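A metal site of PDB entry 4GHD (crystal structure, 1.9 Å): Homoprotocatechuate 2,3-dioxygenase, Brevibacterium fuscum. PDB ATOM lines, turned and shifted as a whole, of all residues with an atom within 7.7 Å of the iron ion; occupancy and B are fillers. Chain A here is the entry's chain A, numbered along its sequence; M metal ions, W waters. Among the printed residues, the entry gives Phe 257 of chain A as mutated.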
ATOM      1  N   ASP A 154     -22.231   0.598 -15.039  1.00  0.00           N
ATOM      2  CA  ASP A 154     -23.122   1.057 -16.125  1.00  0.00           C
ATOM      3  C   ASP A 154     -24.513   1.493 -15.655  1.00  0.00           C
ATOM      4  O   ASP A 154     -24.998   2.509 -16.106  1.00  0.00           O
ATOM      5  CB  ASP A 154     -23.289   0.018 -17.239  1.00  0.00           C
ATOM      6  CG  ASP A 154     -23.985   0.606 -18.501  1.00  0.00           C
ATOM      7  OD1 ASP A 154     -23.315   1.315 -19.283  1.00  0.00           O
ATOM      8  OD2 ASP A 154     -25.222   0.412 -18.680  1.00  0.00           O
ATOM      9  N   HIS A 155     -25.190   0.671 -14.866  1.00  0.00           N
ATOM     10  CA  HIS A 155     -26.568   1.002 -14.474  1.00  0.00           C
ATOM     11  C   HIS A 155     -27.074   0.199 -13.349  1.00  0.00           C
ATOM     12  O   HIS A 155     -26.472  -0.768 -12.950  1.00  0.00           O
ATOM     13  CB  HIS A 155     -27.505   0.787 -15.655  1.00  0.00           C
ATOM     14  CG  HIS A 155     -27.574  -0.626 -16.126  1.00  0.00           C
ATOM     15  ND1 HIS A 155     -26.858  -1.053 -17.168  1.00  0.00           N
ATOM     16  CD2 HIS A 155     -28.312  -1.722 -15.670  1.00  0.00           C
ATOM     17  CE1 HIS A 155     -27.138  -2.358 -17.385  1.00  0.00           C
ATOM     18  NE2 HIS A 155     -28.037  -2.746 -16.491  1.00  0.00           N
ATOM     19  N   PHE A 156     -28.231   0.628 -12.849  1.00  0.00           N
ATOM     20  CA  PHE A 156     -29.076  -0.083 -11.901  1.00  0.00           C
ATOM     21  C   PHE A 156     -30.356  -0.569 -12.611  1.00  0.00           C
ATOM     22  O   PHE A 156     -30.735  -0.037 -13.697  1.00  0.00           O
ATOM     23  CB  PHE A 156     -29.515   0.876 -10.789  1.00  0.00           C
ATOM     24  CG  PHE A 156     -28.384   1.629 -10.102  1.00  0.00           C
ATOM     25  CD1 PHE A 156     -27.282   0.953  -9.546  1.00  0.00           C
ATOM     26  CD2 PHE A 156     -28.440   2.998  -9.998  1.00  0.00           C
ATOM     27  CE1 PHE A 156     -26.257   1.663  -8.928  1.00  0.00           C
ATOM     28  CE2 PHE A 156     -27.410   3.717  -9.402  1.00  0.00           C
ATOM     29  CZ  PHE A 156     -26.332   3.048  -8.852  1.00  0.00           C
ATOM     30  N   ASN A 157     -31.034  -1.567 -12.066  1.00  0.00           N
ATOM     31  CA  ASN A 157     -32.351  -1.938 -12.597  1.00  0.00           C
ATOM     32  C   ASN A 157     -33.219  -2.200 -11.359  1.00  0.00           C
ATOM     33  O   ASN A 157     -32.824  -2.956 -10.508  1.00  0.00           O
ATOM     34  CB  ASN A 157     -32.273  -3.175 -13.492  1.00  0.00           C
ATOM     35  CG  ASN A 157     -33.577  -3.568 -14.108  1.00  0.00           C
ATOM     36  OD1 ASN A 157     -34.563  -3.790 -13.419  1.00  0.00           O
ATOM     37  ND2 ASN A 157     -33.594  -3.717 -15.453  1.00  0.00           N
ATOM     38  N   TRP A 192     -36.321   1.447 -19.846  1.00  0.00           N
ATOM     39  CA  TRP A 192     -34.944   1.800 -19.637  1.00  0.00           C
ATOM     40  C   TRP A 192     -34.809   3.280 -19.821  1.00  0.00           C
ATOM     41  O   TRP A 192     -35.393   3.856 -20.748  1.00  0.00           O
ATOM     42  CB  TRP A 192     -34.100   1.061 -20.680  1.00  0.00           C
ATOM     43  CG  TRP A 192     -33.927  -0.408 -20.387  1.00  0.00           C
ATOM     44  CD1 TRP A 192     -32.829  -1.034 -19.856  1.00  0.00           C
ATOM     45  CD2 TRP A 192     -34.915  -1.483 -20.571  1.00  0.00           C
ATOM     46  NE1 TRP A 192     -33.038  -2.387 -19.697  1.00  0.00           N
ATOM     47  CE2 TRP A 192     -34.267  -2.725 -20.122  1.00  0.00           C
ATOM     48  CE3 TRP A 192     -36.213  -1.543 -21.067  1.00  0.00           C
ATOM     49  CZ2 TRP A 192     -34.907  -3.963 -20.166  1.00  0.00           C
ATOM     50  CZ3 TRP A 192     -36.859  -2.782 -21.104  1.00  0.00           C
ATOM     51  CH2 TRP A 192     -36.216  -3.964 -20.666  1.00  0.00           C
ATOM     52  N   HIS A 200     -29.019   3.280 -20.609  1.00  0.00           N
ATOM     53  CA  HIS A 200     -29.586   3.545 -19.295  1.00  0.00           C
ATOM     54  C   HIS A 200     -28.606   3.764 -18.195  1.00  0.00           C
ATOM     55  O   HIS A 200     -27.484   3.273 -18.227  1.00  0.00           O
ATOM     56  CB  HIS A 200     -30.631   2.504 -18.861  1.00  0.00           C
ATOM     57  CG  HIS A 200     -30.172   1.061 -18.849  1.00  0.00           C
ATOM     58  ND1 HIS A 200     -29.432   0.509 -19.856  1.00  0.00           N
ATOM     59  CD2 HIS A 200     -30.443   0.024 -17.941  1.00  0.00           C
ATOM     60  CE1 HIS A 200     -29.213  -0.809 -19.561  1.00  0.00           C
ATOM     61  NE2 HIS A 200     -29.844  -1.104 -18.412  1.00  0.00           N
ATOM     62  N   ALA A 203     -33.302   1.451 -14.818  1.00  0.00           N
ATOM     63  CA  ALA A 203     -34.377   0.818 -15.552  1.00  0.00           C
ATOM     64  C   ALA A 203     -35.441   0.397 -14.525  1.00  0.00           C
ATOM     65  O   ALA A 203     -35.137   0.162 -13.342  1.00  0.00           O
ATOM     66  CB  ALA A 203     -33.875  -0.406 -16.316  1.00  0.00           C
ATOM     67  N   THR A 205     -38.347  -2.500 -13.932  1.00  0.00           N
ATOM     68  CA  THR A 205     -38.851  -3.823 -14.305  1.00  0.00           C
ATOM     69  C   THR A 205     -40.122  -4.009 -13.488  1.00  0.00           C
ATOM     70  O   THR A 205     -40.094  -3.814 -12.274  1.00  0.00           O
ATOM     71  CB  THR A 205     -37.870  -4.948 -13.939  1.00  0.00           C
ATOM     72  OG1 THR A 205     -36.671  -4.771 -14.673  1.00  0.00           O
ATOM     73  CG2 THR A 205     -38.482  -6.358 -14.229  1.00  0.00           C
ATOM     74  N   HIS A 213     -33.315  -5.131  -8.845  1.00  0.00           N
ATOM     75  CA  HIS A 213     -33.090  -6.258  -9.721  1.00  0.00           C
ATOM     76  C   HIS A 213     -31.636  -6.644  -9.878  1.00  0.00           C
ATOM     77  O   HIS A 213     -31.277  -7.821  -9.701  1.00  0.00           O
ATOM     78  CB  HIS A 213     -33.726  -6.042 -11.075  1.00  0.00           C
ATOM     79  CG  HIS A 213     -33.916  -7.317 -11.782  1.00  0.00           C
ATOM     80  ND1 HIS A 213     -32.916  -7.907 -12.475  1.00  0.00           N
ATOM     81  CD2 HIS A 213     -34.980  -8.212 -11.775  1.00  0.00           C
ATOM     82  CE1 HIS A 213     -33.351  -9.091 -12.947  1.00  0.00           C
ATOM     83  NE2 HIS A 213     -34.619  -9.277 -12.513  1.00  0.00           N
ATOM     84  N   HIS A 214     -30.814  -5.673 -10.288  1.00  0.00           N
ATOM     85  CA  HIS A 214     -29.396  -5.879 -10.392  1.00  0.00           C
ATOM     86  C   HIS A 214     -28.650  -4.587 -10.449  1.00  0.00           C
ATOM     87  O   HIS A 214     -29.231  -3.503 -10.658  1.00  0.00           O
ATOM     88  CB  HIS A 214     -29.082  -6.746 -11.616  1.00  0.00           C
ATOM     89  CG  HIS A 214     -29.571  -6.216 -12.943  1.00  0.00           C
ATOM     90  ND1 HIS A 214     -30.751  -6.593 -13.489  1.00  0.00           N
ATOM     91  CD2 HIS A 214     -28.979  -5.366 -13.857  1.00  0.00           C
ATOM     92  CE1 HIS A 214     -30.901  -5.974 -14.685  1.00  0.00           C
ATOM     93  NE2 HIS A 214     -29.837  -5.244 -14.909  1.00  0.00           N
ATOM     94  N   VAL A 215     -27.323  -4.705 -10.305  1.00  0.00           N
ATOM     95  CA  VAL A 215     -26.378  -3.653 -10.586  1.00  0.00           C
ATOM     96  C   VAL A 215     -25.508  -4.151 -11.767  1.00  0.00           C
ATOM     97  O   VAL A 215     -25.187  -5.339 -11.849  1.00  0.00           O
ATOM     98  CB  VAL A 215     -25.482  -3.390  -9.342  1.00  0.00           C
ATOM     99  CG1 VAL A 215     -24.368  -2.413  -9.669  1.00  0.00           C
ATOM    100  CG2 VAL A 215     -26.321  -2.879  -8.198  1.00  0.00           C
ATOM    101  N   ALA A 216     -25.130  -3.268 -12.678  1.00  0.00           N
ATOM    102  CA  ALA A 216     -24.448  -3.742 -13.914  1.00  0.00           C
ATOM    103  C   ALA A 216     -23.116  -3.053 -14.107  1.00  0.00           C
ATOM    104  O   ALA A 216     -23.017  -1.818 -13.989  1.00  0.00           O
ATOM    105  CB  ALA A 216     -25.355  -3.538 -15.146  1.00  0.00           C
ATOM    106  N   HIS A 248     -28.700  -9.117 -25.650  1.00  0.00           N
ATOM    107  CA  HIS A 248     -29.971  -8.508 -25.389  1.00  0.00           C
ATOM    108  C   HIS A 248     -30.619  -8.048 -26.703  1.00  0.00           C
ATOM    109  O   HIS A 248     -29.933  -7.608 -27.616  1.00  0.00           O
ATOM    110  CB  HIS A 248     -29.825  -7.283 -24.513  1.00  0.00           C
ATOM    111  CG  HIS A 248     -29.639  -7.554 -23.037  1.00  0.00           C
ATOM    112  ND1 HIS A 248     -30.458  -8.375 -22.318  1.00  0.00           N
ATOM    113  CD2 HIS A 248     -28.688  -7.047 -22.146  1.00  0.00           C
ATOM    114  CE1 HIS A 248     -30.034  -8.389 -21.021  1.00  0.00           C
ATOM    115  NE2 HIS A 248     -28.965  -7.557 -20.911  1.00  0.00           N
ATOM    116  N   SER A 251     -31.454  -2.841 -25.714  1.00  0.00           N
ATOM    117  CA  SER A 251     -30.085  -2.322 -25.416  1.00  0.00           C
ATOM    118  C   SER A 251     -29.049  -2.801 -26.438  1.00  0.00           C
ATOM    119  O   SER A 251     -28.015  -2.165 -26.603  1.00  0.00           O
ATOM    120  CB  SER A 251     -29.575  -2.619 -24.006  1.00  0.00           C
ATOM    121  OG  SER A 251     -29.017  -3.925 -23.881  1.00  0.00           O
ATOM    122  N   TYR A 255     -24.361  -9.626 -22.623  1.00  0.00           N
ATOM    123  CA  TYR A 255     -24.636  -9.668 -21.191  1.00  0.00           C
ATOM    124  C   TYR A 255     -24.441 -11.030 -20.523  1.00  0.00           C
ATOM    125  O   TYR A 255     -24.341 -12.057 -21.192  1.00  0.00           O
ATOM    126  CB  TYR A 255     -26.093  -9.226 -20.938  1.00  0.00           C
ATOM    127  CG  TYR A 255     -27.108 -10.295 -21.291  1.00  0.00           C
ATOM    128  CD1 TYR A 255     -27.653 -10.363 -22.568  1.00  0.00           C
ATOM    129  CD2 TYR A 255     -27.468 -11.247 -20.398  1.00  0.00           C
ATOM    130  CE1 TYR A 255     -28.573 -11.354 -22.911  1.00  0.00           C
ATOM    131  CE2 TYR A 255     -28.401 -12.239 -20.726  1.00  0.00           C
ATOM    132  CZ  TYR A 255     -28.925 -12.292 -21.984  1.00  0.00           C
ATOM    133  OH  TYR A 255     -29.825 -13.278 -22.321  1.00  0.00           O
ATOM    134  N   PHE A 257     -25.774 -12.570 -16.405  1.00  0.00           N
ATOM    135  CA  PHE A 257     -26.255 -12.356 -15.007  1.00  0.00           C
ATOM    136  C   PHE A 257     -25.697 -13.463 -14.051  1.00  0.00           C
ATOM    137  O   PHE A 257     -25.858 -14.676 -14.287  1.00  0.00           O
ATOM    138  CB  PHE A 257     -27.767 -12.424 -14.972  1.00  0.00           C
ATOM    139  CG  PHE A 257     -28.428 -11.303 -15.711  1.00  0.00           C
ATOM    140  CD1 PHE A 257     -28.577 -10.065 -15.117  1.00  0.00           C
ATOM    141  CD2 PHE A 257     -28.899 -11.489 -16.963  1.00  0.00           C
ATOM    142  CE1 PHE A 257     -29.177  -9.021 -15.797  1.00  0.00           C
ATOM    143  CE2 PHE A 257     -29.515 -10.438 -17.657  1.00  0.00           C
ATOM    144  CZ  PHE A 257     -29.640  -9.228 -17.084  1.00  0.00           C
ATOM    145  N   GLU A 267     -25.156  -7.873 -13.209  1.00  0.00           N
ATOM    146  CA  GLU A 267     -25.026  -8.031 -14.654  1.00  0.00           C
ATOM    147  C   GLU A 267     -23.648  -7.583 -15.112  1.00  0.00           C
ATOM    148  O   GLU A 267     -23.137  -6.548 -14.642  1.00  0.00           O
ATOM    149  CB  GLU A 267     -26.092  -7.176 -15.373  1.00  0.00           C
ATOM    150  CG  GLU A 267     -26.175  -7.486 -16.846  1.00  0.00           C
ATOM    151  CD  GLU A 267     -27.203  -6.656 -17.601  1.00  0.00           C
ATOM    152  OE1 GLU A 267     -27.650  -5.669 -17.051  1.00  0.00           O
ATOM    153  OE2 GLU A 267     -27.481  -6.965 -18.764  1.00  0.00           O
ATOM    154  N   ILE A 268     -23.061  -8.332 -16.047  1.00  0.00           N
ATOM    155  CA  ILE A 268     -21.916  -7.873 -16.825  1.00  0.00           C
ATOM    156  C   ILE A 268     -22.484  -7.564 -18.204  1.00  0.00           C
ATOM    157  O   ILE A 268     -23.311  -8.332 -18.709  1.00  0.00           O
ATOM    158  CB  ILE A 268     -20.749  -8.905 -16.874  1.00  0.00           C
ATOM    159  CG1 ILE A 268     -20.651  -9.680 -15.565  1.00  0.00           C
ATOM    160  CG2 ILE A 268     -19.409  -8.245 -17.236  1.00  0.00           C
ATOM    161  CD1 ILE A 268     -20.363  -8.877 -14.343  1.00  0.00           C
ATOM    162  N   TYR A 269     -22.047  -6.449 -18.800  1.00  0.00           N
ATOM    163  CA  TYR A 269     -22.716  -5.798 -19.926  1.00  0.00           C
ATOM    164  C   TYR A 269     -21.694  -5.133 -20.817  1.00  0.00           C
ATOM    165  O   TYR A 269     -20.771  -4.501 -20.323  1.00  0.00           O
ATOM    166  CB  TYR A 269     -23.633  -4.759 -19.288  1.00  0.00           C
ATOM    167  CG  TYR A 269     -24.523  -3.888 -20.118  1.00  0.00           C
ATOM    168  CD1 TYR A 269     -25.866  -4.213 -20.296  1.00  0.00           C
ATOM    169  CD2 TYR A 269     -24.069  -2.674 -20.636  1.00  0.00           C
ATOM    170  CE1 TYR A 269     -26.714  -3.397 -20.975  1.00  0.00           C
ATOM    171  CE2 TYR A 269     -24.929  -1.831 -21.338  1.00  0.00           C
ATOM    172  CZ  TYR A 269     -26.256  -2.202 -21.492  1.00  0.00           C
ATOM    173  OH  TYR A 269     -27.126  -1.380 -22.164  1.00  0.00           O
ATOM    174  N   ARG A 293     -35.513  -9.998 -24.935  1.00  0.00           N
ATOM    175  CA  ARG A 293     -34.613 -10.035 -23.785  1.00  0.00           C
ATOM    176  C   ARG A 293     -33.311 -10.734 -24.133  1.00  0.00           C
ATOM    177  O   ARG A 293     -32.262 -10.191 -23.818  1.00  0.00           O
ATOM    178  CB  ARG A 293     -35.248 -10.683 -22.570  1.00  0.00           C
ATOM    179  CG  ARG A 293     -36.221  -9.723 -21.896  1.00  0.00           C
ATOM    180  CD  ARG A 293     -36.656 -10.143 -20.523  1.00  0.00           C
ATOM    181  NE  ARG A 293     -37.549  -9.142 -19.934  1.00  0.00           N
ATOM    182  CZ  ARG A 293     -37.155  -7.993 -19.408  1.00  0.00           C
ATOM    183  NH1 ARG A 293     -35.863  -7.635 -19.378  1.00  0.00           N
ATOM    184  NH2 ARG A 293     -38.063  -7.201 -18.854  1.00  0.00           N
ATOM    185  N   TRP A 304     -35.124 -15.192 -12.732  1.00  0.00           N
ATOM    186  CA  TRP A 304     -34.772 -13.872 -13.194  1.00  0.00           C
ATOM    187  C   TRP A 304     -35.903 -12.906 -13.015  1.00  0.00           C
ATOM    188  O   TRP A 304     -35.692 -11.730 -12.672  1.00  0.00           O
ATOM    189  CB  TRP A 304     -34.311 -13.921 -14.673  1.00  0.00           C
ATOM    190  CG  TRP A 304     -33.624 -12.650 -15.102  1.00  0.00           C
ATOM    191  CD1 TRP A 304     -32.278 -12.381 -15.034  1.00  0.00           C
ATOM    192  CD2 TRP A 304     -34.244 -11.438 -15.636  1.00  0.00           C
ATOM    193  NE1 TRP A 304     -32.035 -11.120 -15.465  1.00  0.00           N
ATOM    194  CE2 TRP A 304     -33.158 -10.500 -15.846  1.00  0.00           C
ATOM    195  CE3 TRP A 304     -35.529 -11.047 -15.942  1.00  0.00           C
ATOM    196  CZ2 TRP A 304     -33.367  -9.220 -16.309  1.00  0.00           C
ATOM    197  CZ3 TRP A 304     -35.726  -9.755 -16.407  1.00  0.00           C
ATOM    198  CH2 TRP A 304     -34.652  -8.869 -16.606  1.00  0.00           C
HETATM  199 FE    FE M   1     -29.424  -4.561 -16.965  1.00  0.00          FE
HETATM  200  O   HOH W   1     -29.577  -4.774 -19.193  1.00  0.00           O
HETATM  201  O   HOH W   2     -31.366  -6.088 -18.143  1.00  0.00           O
HETATM  202  O   HOH W   3     -31.293  -3.167 -17.092  1.00  0.00           O
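Water W3 lies within hydrogen-bond range of NE2 of His 200, ND2 of Asn 157 and NE1 of Trp 192.
Water W1 bridges the side-chain carboxylate of Glu 267 and a ring nitrogen (NE2) of His 248.
A ring nitrogen (NE2) of His 248 is in hydrogen-bond range of the side-chain carboxylate (OE2) of Glu 267 (2.7 Å).
The backbone NH (N) of Glu 267 lies within hydrogen-bond range of the backbone carbonyl oxygen (O) of Val 215 (2.9 Å).
The backbone carbonyl oxygen (O) of His 214 lies within hydrogen-bond range of the backbone NH (N) of Asn 157, 3.0 Å away.
A ring nitrogen (ND1) of His 213 is in hydrogen-bond range of a ring nitrogen (ND1) of His 214 (2.7 Å).
A ring nitrogen (NE2) of His 200 lies close to a ring nitrogen (ND1) of His 155, at 3.2 Å.
The backbone carbonyl oxygen of His 155 sits at hydrogen-bond distance from the backbone NH of Ala 216, at 2.9 Å.
The side-chain carboxylate (OD2) of Asp 154 sits at hydrogen-bond distance from a ring nitrogen (ND1) of His 155, at 2.7 Å.
Residues that only touch the iron ion: His 200 (3.8 Å).
Within 4 Å of the iron ion: His 155, His 200, His 214 and Glu 267.
OE1 of Glu 267 is bound to the iron ion, 2.1 Å away.
NE2 of His 214 is bound to the iron ion, 2.2 Å away.
Water W1 is bound to the iron ion.
NE2 of His 155 is bound to the iron ion, at 2.3 Å.
The iron ion is bound by water W3 (2.3 Å).
Slightly farther from the iron ion lies water W2 (2.7 Å).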
